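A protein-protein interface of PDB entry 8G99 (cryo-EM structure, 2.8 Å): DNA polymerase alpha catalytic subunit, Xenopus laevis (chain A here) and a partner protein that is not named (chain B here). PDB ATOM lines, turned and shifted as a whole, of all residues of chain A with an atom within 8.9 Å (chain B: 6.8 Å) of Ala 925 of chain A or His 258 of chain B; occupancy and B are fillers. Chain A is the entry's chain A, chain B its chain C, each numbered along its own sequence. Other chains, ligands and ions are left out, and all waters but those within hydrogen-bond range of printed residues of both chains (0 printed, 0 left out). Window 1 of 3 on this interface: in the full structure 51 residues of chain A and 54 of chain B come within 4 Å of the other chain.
The side-chain carboxylate of Asp 924 of chain A lies within salt-bridge range of the guanidinium group of Arg 365 of chain B (2.9 Å).
The side-chain amide nitrogen of Gln 932 of chain A sits at hydrogen-bond distance from the backbone carbonyl oxygen of Tyr 263 of chain B (2.9 Å).
The backbone carbonyl oxygen (O) of Leu 927 of chain A sits at hydrogen-bond distance from the guanidinium group (NH2) of Arg 365 of chain B (3.3 Å).
The backbone NH (N) of Leu 926 of chain A lies within hydrogen-bond range of the backbone carbonyl oxygen (O) of His 261 of chain B, 3.4 Å away.
The backbone carbonyl oxygen (O) of Ala 925 of chain A lies close to the backbone carbonyl oxygen (O) of His 261 of chain B, 3.3 Å away.
The backbone carbonyl oxygen (O) of Ala 925 of chain A is in hydrogen-bond range of the backbone NH (N) of Tyr 263 of chain B.
O of Leu 926 of chain A sits at hydrogen-bond distance from OG of Ser 372 of chain B, at 2.6 Å.
The side-chain amide nitrogen (NE2) of Gln 932 of chain A lies close to the backbone carbonyl oxygen (O) of Gly 928 of chain A, 3.3 Å away.
The side-chain carboxylate (OD1) of Asp 924 of chain A sits close to the backbone carbonyl oxygen (O) of Asp 920 of chain A (2.7 Å).
The side-chain amino group (NZ) of Lys 516 of chain A is in salt-bridge range of the side-chain carboxylate (OE1) of Glu 922 of chain A, at 3.4 Å.
O of Leu 259 of chain B lies close to OG of Ser 262 of chain B (3.2 Å).
The side-chain hydroxyl of Ser 262 of chain B is in hydrogen-bond range of the backbone carbonyl oxygen of His 258 of chain B.
The backbone carbonyl oxygen of Asp 924 of chain A sits at hydrogen-bond distance from the backbone NH of Gly 929 of chain A.
Glu 921 of chain A touches Pro 254 of chain B.
Glu 921 of chain A touches His 258 of chain B.
Glu 922 of chain A touches His 258 of chain B (N to CE1, 3.8 Å).
Ala 925 of chain A touches Ser 262 of chain B.
Leu 926 of chain A touches Tyr 263 of chain B.
Leu 926 of chain A touches Met 374 of chain B (CD2 to O, 3.9 Å).
O of Leu 927 of chain A touches CD2 of Tyr 263 of chain B (3.8 Å).
Tyr 263 of chain B touches Gly 928 of chain A (CB to N, 3.6 Å).
Arg 365 of chain B touches Gly 929 of chain A.
Arg 365 of chain B touches Leu 933 of chain A (NH2 to CD2, 3.1 Å).
Of the printed residues of chain B, Glu 922 of chain A touches His 258 (3.8 Å).
Of chain B, only His 258 (3.7 Å), His 261 (3.3 Å), Ser 262 (3.3 Å) and Tyr 263 (2.8 Å) come within 4 Å of Ala 925 of chain A.
Of the printed residues of chain A, His 258 of chain B touches Glu 921, Glu 922 and Ala 925.
Of chain A, only Ala 925 (3.3 Å) comes within 4 Å of Ser 262 of chain B.
Of the printed residues of chain A, Tyr 263 of chain B touches Ala 925 (2.8 Å), Leu 926 (3.3 Å), Leu 927 (3.8 Å), Gly 928 (3.6 Å) and Gln 932 (2.9 Å).
The nearest residue of chain B that does not touch Ala 925 of chain A is Met 374 of chain B (4.6 Å).
The nearest residue of chain A that does not touch His 258 of chain B is Lys 653 of chain A (5.8 Å).
The nearest printed residue of chain B that does not touch Leu 926 of chain A is Ser 262 of chain B (4.9 Å).
Of the 19 printed residues of chain A, 12 touch a printed residue of chain B.
Hydrophobic or aromatic side chains of chain A within 4 Å of the printed part of chain B: Leu 650, Ala 925, Leu 926, Leu 927 and Leu 933.
Hydrophobic or aromatic side chains of chain B that line the printed part of chain A: Pro 254, Leu 255, His 258 and Tyr 263.
Among the printed residues, 21 pairs touch across the chains.
Among the printed residues, Asp or Glu carboxylates within 4 Å of a Lys or Arg side-chain nitrogen of the other chain: Asp 924 of chain A with Arg 365 of chain B.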
ATOM      1  N   LEU A 513      26.297  29.253  -3.017  1.00  0.00           N
ATOM      2  CA  LEU A 513      26.807  27.887  -2.982  1.00  0.00           C
ATOM      3  C   LEU A 513      28.230  27.968  -2.451  1.00  0.00           C
ATOM      4  O   LEU A 513      29.152  28.361  -3.168  1.00  0.00           O
ATOM      5  CB  LEU A 513      26.747  27.249  -4.364  1.00  0.00           C
ATOM      6  CG  LEU A 513      25.376  27.287  -5.045  1.00  0.00           C
ATOM      7  CD1 LEU A 513      25.479  26.847  -6.493  1.00  0.00           C
ATOM      8  CD2 LEU A 513      24.379  26.423  -4.292  1.00  0.00           C
ATOM      9  N   GLU A 514      28.411  27.601  -1.186  1.00  0.00           N
ATOM     10  CA  GLU A 514      29.659  27.890  -0.503  1.00  0.00           C
ATOM     11  C   GLU A 514      30.827  27.238  -1.239  1.00  0.00           C
ATOM     12  O   GLU A 514      30.677  26.170  -1.837  1.00  0.00           O
ATOM     13  CB  GLU A 514      29.606  27.395   0.941  1.00  0.00           C
ATOM     14  CG  GLU A 514      29.242  25.919   1.090  1.00  0.00           C
ATOM     15  CD  GLU A 514      30.434  25.036   1.425  1.00  0.00           C
ATOM     16  OE1 GLU A 514      31.544  25.568   1.641  1.00  0.00           O
ATOM     17  OE2 GLU A 514      30.257  23.800   1.472  1.00  0.00           O
ATOM     18  N   LYS A 516      33.798  25.061  -2.504  1.00  0.00           N
ATOM     19  CA  LYS A 516      34.238  23.694  -2.246  1.00  0.00           C
ATOM     20  C   LYS A 516      35.760  23.720  -2.206  1.00  0.00           C
ATOM     21  O   LYS A 516      36.437  23.482  -3.204  1.00  0.00           O
ATOM     22  CB  LYS A 516      33.699  22.750  -3.313  1.00  0.00           C
ATOM     23  CG  LYS A 516      33.663  21.296  -2.893  1.00  0.00           C
ATOM     24  CD  LYS A 516      33.296  20.386  -4.057  1.00  0.00           C
ATOM     25  CE  LYS A 516      31.920  20.709  -4.625  1.00  0.00           C
ATOM     26  NZ  LYS A 516      30.877  20.822  -3.569  1.00  0.00           N
ATOM     27  N   LEU A 650      19.817  26.865  -7.684  1.00  0.00           N
ATOM     28  CA  LEU A 650      19.778  25.470  -7.257  1.00  0.00           C
ATOM     29  C   LEU A 650      19.519  24.539  -8.436  1.00  0.00           C
ATOM     30  O   LEU A 650      20.131  23.466  -8.540  1.00  0.00           O
ATOM     31  CB  LEU A 650      18.720  25.282  -6.173  1.00  0.00           C
ATOM     32  CG  LEU A 650      19.106  25.802  -4.786  1.00  0.00           C
ATOM     33  CD1 LEU A 650      17.890  25.869  -3.882  1.00  0.00           C
ATOM     34  CD2 LEU A 650      20.186  24.939  -4.158  1.00  0.00           C
ATOM     35  N   LYS A 653      22.690  24.122 -10.352  1.00  0.00           N
ATOM     36  CA  LYS A 653      23.562  23.170  -9.674  1.00  0.00           C
ATOM     37  C   LYS A 653      23.137  21.740  -9.971  1.00  0.00           C
ATOM     38  O   LYS A 653      23.976  20.883 -10.271  1.00  0.00           O
ATOM     39  CB  LYS A 653      23.554  23.423  -8.168  1.00  0.00           C
ATOM     40  CG  LYS A 653      24.725  22.790  -7.440  1.00  0.00           C
ATOM     41  CD  LYS A 653      24.506  22.765  -5.942  1.00  0.00           C
ATOM     42  CE  LYS A 653      25.649  22.069  -5.229  1.00  0.00           C
ATOM     43  NZ  LYS A 653      25.554  22.205  -3.749  1.00  0.00           N
ATOM     44  N   ASP A 920      33.320  19.939   5.611  1.00  0.00           N
ATOM     45  CA  ASP A 920      32.220  20.177   4.685  1.00  0.00           C
ATOM     46  C   ASP A 920      30.966  19.438   5.136  1.00  0.00           C
ATOM     47  O   ASP A 920      31.025  18.270   5.515  1.00  0.00           O
ATOM     48  CB  ASP A 920      32.605  19.742   3.270  1.00  0.00           C
ATOM     49  CG  ASP A 920      33.671  20.627   2.657  1.00  0.00           C
ATOM     50  OD1 ASP A 920      33.917  21.727   3.197  1.00  0.00           O
ATOM     51  OD2 ASP A 920      34.265  20.224   1.634  1.00  0.00           O
ATOM     52  N   GLU A 921      29.828  20.134   5.096  1.00  0.00           N
ATOM     53  CA  GLU A 921      28.572  19.519   5.509  1.00  0.00           C
ATOM     54  C   GLU A 921      28.076  18.507   4.485  1.00  0.00           C
ATOM     55  O   GLU A 921      27.461  17.503   4.859  1.00  0.00           O
ATOM     56  CB  GLU A 921      27.515  20.597   5.742  1.00  0.00           C
ATOM     57  CG  GLU A 921      27.761  21.449   6.978  1.00  0.00           C
ATOM     58  CD  GLU A 921      28.753  22.568   6.729  1.00  0.00           C
ATOM     59  OE1 GLU A 921      29.373  22.589   5.646  1.00  0.00           O
ATOM     60  OE2 GLU A 921      28.911  23.430   7.620  1.00  0.00           O
ATOM     61  N   GLU A 922      28.327  18.751   3.198  1.00  0.00           N
ATOM     62  CA  GLU A 922      27.842  17.839   2.168  1.00  0.00           C
ATOM     63  C   GLU A 922      28.446  16.450   2.337  1.00  0.00           C
ATOM     64  O   GLU A 922      27.737  15.440   2.279  1.00  0.00           O
ATOM     65  CB  GLU A 922      28.162  18.399   0.782  1.00  0.00           C
ATOM     66  CG  GLU A 922      27.473  17.663  -0.353  1.00  0.00           C
ATOM     67  CD  GLU A 922      27.719  18.310  -1.702  1.00  0.00           C
ATOM     68  OE1 GLU A 922      28.465  19.311  -1.755  1.00  0.00           O
ATOM     69  OE2 GLU A 922      27.168  17.819  -2.708  1.00  0.00           O
ATOM     70  N   ASN A 923      29.761  16.382   2.548  1.00  0.00           N
ATOM     71  CA  ASN A 923      30.412  15.086   2.707  1.00  0.00           C
ATOM     72  C   ASN A 923      29.932  14.381   3.967  1.00  0.00           C
ATOM     73  O   ASN A 923      29.765  13.156   3.974  1.00  0.00           O
ATOM     74  CB  ASN A 923      31.928  15.260   2.733  1.00  0.00           C
ATOM     75  CG  ASN A 923      32.501  15.554   1.364  1.00  0.00           C
ATOM     76  OD1 ASN A 923      31.845  15.346   0.345  1.00  0.00           O
ATOM     77  ND2 ASN A 923      33.735  16.041   1.333  1.00  0.00           N
ATOM     78  N   ASP A 924      29.708  15.133   5.044  1.00  0.00           N
ATOM     79  CA  ASP A 924      29.205  14.525   6.269  1.00  0.00           C
ATOM     80  C   ASP A 924      27.849  13.877   6.036  1.00  0.00           C
ATOM     81  O   ASP A 924      27.591  12.767   6.518  1.00  0.00           O
ATOM     82  CB  ASP A 924      29.118  15.574   7.376  1.00  0.00           C
ATOM     83  CG  ASP A 924      30.435  15.773   8.096  1.00  0.00           C
ATOM     84  OD1 ASP A 924      31.270  16.559   7.602  1.00  0.00           O
ATOM     85  OD2 ASP A 924      30.638  15.142   9.155  1.00  0.00           O
ATOM     86  N   ALA A 925      26.967  14.552   5.298  1.00  0.00           N
ATOM     87  CA  ALA A 925      25.675  13.961   4.973  1.00  0.00           C
ATOM     88  C   ALA A 925      25.847  12.703   4.132  1.00  0.00           C
ATOM     89  O   ALA A 925      25.160  11.700   4.353  1.00  0.00           O
ATOM     90  CB  ALA A 925      24.803  14.979   4.242  1.00  0.00           C
ATOM     91  N   LEU A 926      26.766  12.737   3.167  1.00  0.00           N
ATOM     92  CA  LEU A 926      26.985  11.582   2.308  1.00  0.00           C
ATOM     93  C   LEU A 926      27.494  10.374   3.083  1.00  0.00           C
ATOM     94  O   LEU A 926      27.356   9.245   2.604  1.00  0.00           O
ATOM     95  CB  LEU A 926      27.971  11.942   1.199  1.00  0.00           C
ATOM     96  CG  LEU A 926      27.444  12.910   0.138  1.00  0.00           C
ATOM     97  CD1 LEU A 926      28.584  13.517  -0.653  1.00  0.00           C
ATOM     98  CD2 LEU A 926      26.466  12.212  -0.787  1.00  0.00           C
ATOM     99  N   LEU A 927      28.075  10.583   4.263  1.00  0.00           N
ATOM    100  CA  LEU A 927      28.616   9.504   5.076  1.00  0.00           C
ATOM    101  C   LEU A 927      27.785   9.233   6.325  1.00  0.00           C
ATOM    102  O   LEU A 927      28.197   8.428   7.165  1.00  0.00           O
ATOM    103  CB  LEU A 927      30.060   9.819   5.470  1.00  0.00           C
ATOM    104  CG  LEU A 927      31.077   9.776   4.330  1.00  0.00           C
ATOM    105  CD1 LEU A 927      32.413  10.333   4.785  1.00  0.00           C
ATOM    106  CD2 LEU A 927      31.239   8.361   3.805  1.00  0.00           C
ATOM    107  N   GLY A 928      26.630   9.878   6.467  1.00  0.00           N
ATOM    108  CA  GLY A 928      25.767   9.641   7.606  1.00  0.00           C
ATOM    109  C   GLY A 928      25.181  10.910   8.187  1.00  0.00           C
ATOM    110  O   GLY A 928      24.046  10.911   8.674  1.00  0.00           O
ATOM    111  N   GLY A 929      25.941  11.997   8.139  1.00  0.00           N
ATOM    112  CA  GLY A 929      25.489  13.264   8.658  1.00  0.00           C
ATOM    113  C   GLY A 929      25.789  13.416  10.136  1.00  0.00           C
ATOM    114  O   GLY A 929      26.138  12.452  10.823  1.00  0.00           O
ATOM    115  N   PRO A 930      25.656  14.638  10.655  1.00  0.00           N
ATOM    116  CA  PRO A 930      25.947  14.860  12.081  1.00  0.00           C
ATOM    117  C   PRO A 930      25.025  14.101  13.017  1.00  0.00           C
ATOM    118  O   PRO A 930      25.376  13.916  14.189  1.00  0.00           O
ATOM    119  CB  PRO A 930      25.778  16.378  12.247  1.00  0.00           C
ATOM    120  CG  PRO A 930      25.820  16.941  10.865  1.00  0.00           C
ATOM    121  CD  PRO A 930      25.271  15.883   9.971  1.00  0.00           C
ATOM    122  N   SER A 931      23.862  13.660  12.547  1.00  0.00           N
ATOM    123  CA  SER A 931      22.873  13.031  13.410  1.00  0.00           C
ATOM    124  C   SER A 931      23.058  11.527  13.559  1.00  0.00           C
ATOM    125  O   SER A 931      22.386  10.922  14.400  1.00  0.00           O
ATOM    126  CB  SER A 931      21.466  13.305  12.874  1.00  0.00           C
ATOM    127  OG  SER A 931      21.255  14.694  12.686  1.00  0.00           O
ATOM    128  N   GLN A 932      23.942  10.910  12.780  1.00  0.00           N
ATOM    129  CA  GLN A 932      24.126   9.464  12.792  1.00  0.00           C
ATOM    130  C   GLN A 932      25.561   9.093  13.136  1.00  0.00           C
ATOM    131  O   GLN A 932      26.140   8.171  12.557  1.00  0.00           O
ATOM    132  CB  GLN A 932      23.726   8.858  11.449  1.00  0.00           C
ATOM    133  CG  GLN A 932      22.365   9.300  10.951  1.00  0.00           C
ATOM    134  CD  GLN A 932      21.834   8.403   9.856  1.00  0.00           C
ATOM    135  OE1 GLN A 932      21.866   7.179   9.973  1.00  0.00           O
ATOM    136  NE2 GLN A 932      21.342   9.007   8.782  1.00  0.00           N
ATOM    137  N   LEU A 933      26.153   9.804  14.088  1.00  0.00           N
ATOM    138  CA  LEU A 933      27.506   9.511  14.532  1.00  0.00           C
ATOM    139  C   LEU A 933      27.483   8.530  15.695  1.00  0.00           C
ATOM    140  O   LEU A 933      26.535   8.490  16.483  1.00  0.00           O
ATOM    141  CB  LEU A 933      28.228  10.789  14.957  1.00  0.00           C
ATOM    142  CG  LEU A 933      28.199  11.961  13.980  1.00  0.00           C
ATOM    143  CD1 LEU A 933      29.226  13.003  14.382  1.00  0.00           C
ATOM    144  CD2 LEU A 933      28.440  11.492  12.554  1.00  0.00           C
ATOM    145  N   LEU B  52      12.947  10.287   6.401  1.00  0.00           N
ATOM    146  CA  LEU B  52      13.714  10.183   5.165  1.00  0.00           C
ATOM    147  C   LEU B  52      13.904   8.725   4.768  1.00  0.00           C
ATOM    148  O   LEU B  52      13.768   8.369   3.591  1.00  0.00           O
ATOM    149  CB  LEU B  52      15.067  10.874   5.320  1.00  0.00           C
ATOM    150  CG  LEU B  52      15.868  11.024   4.026  1.00  0.00           C
ATOM    151  CD1 LEU B  52      15.288  12.126   3.161  1.00  0.00           C
ATOM    152  CD2 LEU B  52      17.328  11.287   4.332  1.00  0.00           C
ATOM    153  N   ALA B 115      12.895  20.464   4.702  1.00  0.00           N
ATOM    154  CA  ALA B 115      14.015  19.932   3.938  1.00  0.00           C
ATOM    155  C   ALA B 115      13.752  19.930   2.436  1.00  0.00           C
ATOM    156  O   ALA B 115      14.699  20.042   1.652  1.00  0.00           O
ATOM    157  CB  ALA B 115      14.339  18.513   4.402  1.00  0.00           C
ATOM    158  N   GLN B 118      13.290  23.666  -1.182  1.00  0.00           N
ATOM    159  CA  GLN B 118      14.248  24.613  -1.737  1.00  0.00           C
ATOM    160  C   GLN B 118      14.236  24.614  -3.260  1.00  0.00           C
ATOM    161  O   GLN B 118      14.371  25.674  -3.879  1.00  0.00           O
ATOM    162  CB  GLN B 118      15.648  24.291  -1.218  1.00  0.00           C
ATOM    163  CG  GLN B 118      15.888  24.746   0.211  1.00  0.00           C
ATOM    164  CD  GLN B 118      16.453  23.652   1.094  1.00  0.00           C
ATOM    165  OE1 GLN B 118      17.083  22.710   0.613  1.00  0.00           O
ATOM    166  NE2 GLN B 118      16.230  23.773   2.397  1.00  0.00           N
ATOM    167  N   GLN B 253      20.800  23.877   9.837  1.00  0.00           N
ATOM    168  CA  GLN B 253      21.199  24.128   8.458  1.00  0.00           C
ATOM    169  C   GLN B 253      21.900  22.913   7.861  1.00  0.00           C
ATOM    170  O   GLN B 253      21.555  22.493   6.750  1.00  0.00           O
ATOM    171  CB  GLN B 253      22.102  25.357   8.373  1.00  0.00           C
ATOM    172  CG  GLN B 253      21.382  26.603   7.902  1.00  0.00           C
ATOM    173  CD  GLN B 253      21.118  26.593   6.410  1.00  0.00           C
ATOM    174  OE1 GLN B 253      21.971  26.986   5.615  1.00  0.00           O
ATOM    175  NE2 GLN B 253      19.931  26.142   6.021  1.00  0.00           N
ATOM    176  N   PRO B 254      22.880  22.322   8.548  1.00  0.00           N
ATOM    177  CA  PRO B 254      23.534  21.133   7.980  1.00  0.00           C
ATOM    178  C   PRO B 254      22.560  20.024   7.639  1.00  0.00           C
ATOM    179  O   PRO B 254      22.747  19.325   6.635  1.00  0.00           O
ATOM    180  CB  PRO B 254      24.511  20.710   9.085  1.00  0.00           C
ATOM    181  CG  PRO B 254      24.765  21.934   9.861  1.00  0.00           C
ATOM    182  CD  PRO B 254      23.516  22.751   9.802  1.00  0.00           C
ATOM    183  N   LEU B 255      21.520  19.842   8.449  1.00  0.00           N
ATOM    184  CA  LEU B 255      20.558  18.777   8.196  1.00  0.00           C
ATOM    185  C   LEU B 255      19.664  19.119   7.009  1.00  0.00           C
ATOM    186  O   LEU B 255      19.703  18.451   5.969  1.00  0.00           O
ATOM    187  CB  LEU B 255      19.724  18.535   9.455  1.00  0.00           C
ATOM    188  CG  LEU B 255      18.892  17.255   9.514  1.00  0.00           C
ATOM    189  CD1 LEU B 255      19.771  16.042   9.756  1.00  0.00           C
ATOM    190  CD2 LEU B 255      17.832  17.367  10.592  1.00  0.00           C
ATOM    191  N   LEU B 256      18.882  20.191   7.134  1.00  0.00           N
ATOM    192  CA  LEU B 256      17.851  20.478   6.143  1.00  0.00           C
ATOM    193  C   LEU B 256      18.451  20.738   4.768  1.00  0.00           C
ATOM    194  O   LEU B 256      17.909  20.288   3.753  1.00  0.00           O
ATOM    195  CB  LEU B 256      17.011  21.669   6.600  1.00  0.00           C
ATOM    196  CG  LEU B 256      16.341  21.507   7.967  1.00  0.00           C
ATOM    197  CD1 LEU B 256      15.672  22.800   8.393  1.00  0.00           C
ATOM    198  CD2 LEU B 256      15.340  20.368   7.948  1.00  0.00           C
ATOM    199  N   ASN B 257      19.569  21.460   4.709  1.00  0.00           N
ATOM    200  CA  ASN B 257      20.186  21.753   3.423  1.00  0.00           C
ATOM    201  C   ASN B 257      20.730  20.509   2.738  1.00  0.00           C
ATOM    202  O   ASN B 257      20.996  20.553   1.532  1.00  0.00           O
ATOM    203  CB  ASN B 257      21.320  22.764   3.593  1.00  0.00           C
ATOM    204  CG  ASN B 257      20.835  24.197   3.551  1.00  0.00           C
ATOM    205  OD1 ASN B 257      19.648  24.469   3.725  1.00  0.00           O
ATOM    206  ND2 ASN B 257      21.755  25.123   3.317  1.00  0.00           N
ATOM    207  N   HIS B 258      20.907  19.403   3.466  1.00  0.00           N
ATOM    208  CA  HIS B 258      21.565  18.229   2.911  1.00  0.00           C
ATOM    209  C   HIS B 258      20.826  16.930   3.204  1.00  0.00           C
ATOM    210  O   HIS B 258      21.362  15.852   2.924  1.00  0.00           O
ATOM    211  CB  HIS B 258      23.000  18.133   3.439  1.00  0.00           C
ATOM    212  CG  HIS B 258      23.884  19.245   2.973  1.00  0.00           C
ATOM    213  ND1 HIS B 258      24.554  20.076   3.843  1.00  0.00           N
ATOM    214  CD2 HIS B 258      24.203  19.669   1.728  1.00  0.00           C
ATOM    215  CE1 HIS B 258      25.250  20.962   3.154  1.00  0.00           C
ATOM    216  NE2 HIS B 258      25.054  20.737   1.868  1.00  0.00           N
ATOM    217  N   LEU B 259      19.607  16.999   3.739  1.00  0.00           N
ATOM    218  CA  LEU B 259      18.876  15.778   4.055  1.00  0.00           C
ATOM    219  C   LEU B 259      18.720  14.898   2.822  1.00  0.00           C
ATOM    220  O   LEU B 259      18.926  13.680   2.888  1.00  0.00           O
ATOM    221  CB  LEU B 259      17.511  16.130   4.643  1.00  0.00           C
ATOM    222  CG  LEU B 259      16.817  15.043   5.461  1.00  0.00           C
ATOM    223  CD1 LEU B 259      17.509  14.841   6.793  1.00  0.00           C
ATOM    224  CD2 LEU B 259      15.357  15.392   5.669  1.00  0.00           C
ATOM    225  N   SER B 260      18.385  15.500   1.680  1.00  0.00           N
ATOM    226  CA  SER B 260      18.185  14.720   0.465  1.00  0.00           C
ATOM    227  C   SER B 260      19.420  13.909   0.106  1.00  0.00           C
ATOM    228  O   SER B 260      19.310  12.874  -0.558  1.00  0.00           O
ATOM    229  CB  SER B 260      17.806  15.646  -0.688  1.00  0.00           C
ATOM    230  OG  SER B 260      18.771  16.667  -0.858  1.00  0.00           O
ATOM    231  N   HIS B 261      20.598  14.354   0.536  1.00  0.00           N
ATOM    232  CA  HIS B 261      21.854  13.664   0.273  1.00  0.00           C
ATOM    233  C   HIS B 261      22.424  13.050   1.547  1.00  0.00           C
ATOM    234  O   HIS B 261      23.634  13.073   1.778  1.00  0.00           O
ATOM    235  CB  HIS B 261      22.868  14.614  -0.353  1.00  0.00           C
ATOM    236  CG  HIS B 261      22.401  15.237  -1.629  1.00  0.00           C
ATOM    237  ND1 HIS B 261      22.070  14.495  -2.742  1.00  0.00           N
ATOM    238  CD2 HIS B 261      22.218  16.533  -1.973  1.00  0.00           C
ATOM    239  CE1 HIS B 261      21.698  15.307  -3.715  1.00  0.00           C
ATOM    240  NE2 HIS B 261      21.778  16.549  -3.275  1.00  0.00           N
ATOM    241  N   SER B 262      21.559  12.495   2.391  1.00  0.00           N
ATOM    242  CA  SER B 262      21.969  11.916   3.662  1.00  0.00           C
ATOM    243  C   SER B 262      21.994  10.397   3.562  1.00  0.00           C
ATOM    244  O   SER B 262      21.002   9.779   3.162  1.00  0.00           O
ATOM    245  CB  SER B 262      21.029  12.353   4.784  1.00  0.00           C
ATOM    246  OG  SER B 262      21.232  13.716   5.109  1.00  0.00           O
ATOM    247  N   TYR B 263      23.129   9.804   3.922  1.00  0.00           N
ATOM    248  CA  TYR B 263      23.255   8.355   3.930  1.00  0.00           C
ATOM    249  C   TYR B 263      22.459   7.773   5.092  1.00  0.00           C
ATOM    250  O   TYR B 263      22.558   8.250   6.226  1.00  0.00           O
ATOM    251  CB  TYR B 263      24.730   7.966   4.031  1.00  0.00           C
ATOM    252  CG  TYR B 263      24.985   6.509   4.322  1.00  0.00           C
ATOM    253  CD1 TYR B 263      24.512   5.518   3.479  1.00  0.00           C
ATOM    254  CD2 TYR B 263      25.712   6.125   5.437  1.00  0.00           C
ATOM    255  CE1 TYR B 263      24.747   4.190   3.744  1.00  0.00           C
ATOM    256  CE2 TYR B 263      25.951   4.800   5.707  1.00  0.00           C
ATOM    257  CZ  TYR B 263      25.469   3.837   4.858  1.00  0.00           C
ATOM    258  OH  TYR B 263      25.707   2.510   5.125  1.00  0.00           O
ATOM    259  N   ILE B 264      21.669   6.738   4.810  1.00  0.00           N
ATOM    260  CA  ILE B 264      20.710   6.214   5.776  1.00  0.00           C
ATOM    261  C   ILE B 264      20.958   4.735   6.048  1.00  0.00           C
ATOM    262  O   ILE B 264      20.027   3.993   6.374  1.00  0.00           O
ATOM    263  CB  ILE B 264      19.270   6.432   5.281  1.00  0.00           C
ATOM    264  CG1 ILE B 264      19.078   5.800   3.901  1.00  0.00           C
ATOM    265  CG2 ILE B 264      18.949   7.914   5.230  1.00  0.00           C
ATOM    266  CD1 ILE B 264      17.639   5.747   3.453  1.00  0.00           C
ATOM    267  N   ARG B 365      36.709  12.916   8.635  1.00  0.00           N
ATOM    268  CA  ARG B 365      35.645  11.915   8.627  1.00  0.00           C
ATOM    269  C   ARG B 365      35.421  11.320   7.242  1.00  0.00           C
ATOM    270  O   ARG B 365      34.681  10.342   7.098  1.00  0.00           O
ATOM    271  CB  ARG B 365      34.334  12.511   9.149  1.00  0.00           C
ATOM    272  CG  ARG B 365      33.197  11.513   9.195  1.00  0.00           C
ATOM    273  CD  ARG B 365      32.254  11.792  10.340  1.00  0.00           C
ATOM    274  NE  ARG B 365      31.090  10.916  10.302  1.00  0.00           N
ATOM    275  CZ  ARG B 365      29.958  11.194   9.670  1.00  0.00           C
ATOM    276  NH1 ARG B 365      29.798  12.324   8.998  1.00  0.00           N
ATOM    277  NH2 ARG B 365      28.960  10.317   9.710  1.00  0.00           N
ATOM    278  N   SER B 372      30.151   5.455   1.163  1.00  0.00           N
ATOM    279  CA  SER B 372      28.851   4.876   0.877  1.00  0.00           C
ATOM    280  C   SER B 372      28.508   5.055  -0.596  1.00  0.00           C
ATOM    281  O   SER B 372      29.125   5.843  -1.316  1.00  0.00           O
ATOM    282  CB  SER B 372      27.777   5.515   1.753  1.00  0.00           C
ATOM    283  OG  SER B 372      27.652   6.895   1.468  1.00  0.00           O
ATOM    284  N   MET B 374      26.102   6.571  -2.073  1.00  0.00           N
ATOM    285  CA  MET B 374      25.856   7.964  -2.416  1.00  0.00           C
ATOM    286  C   MET B 374      27.160   8.746  -2.480  1.00  0.00           C
ATOM    287  O   MET B 374      27.388   9.506  -3.426  1.00  0.00           O
ATOM    288  CB  MET B 374      24.892   8.587  -1.411  1.00  0.00           C
ATOM    289  CG  MET B 374      23.440   8.494  -1.850  1.00  0.00           C
ATOM    290  SD  MET B 374      22.237   9.157  -0.687  1.00  0.00           S
ATOM    291  CE  MET B 374      23.282  10.042   0.462  1.00  0.00           C
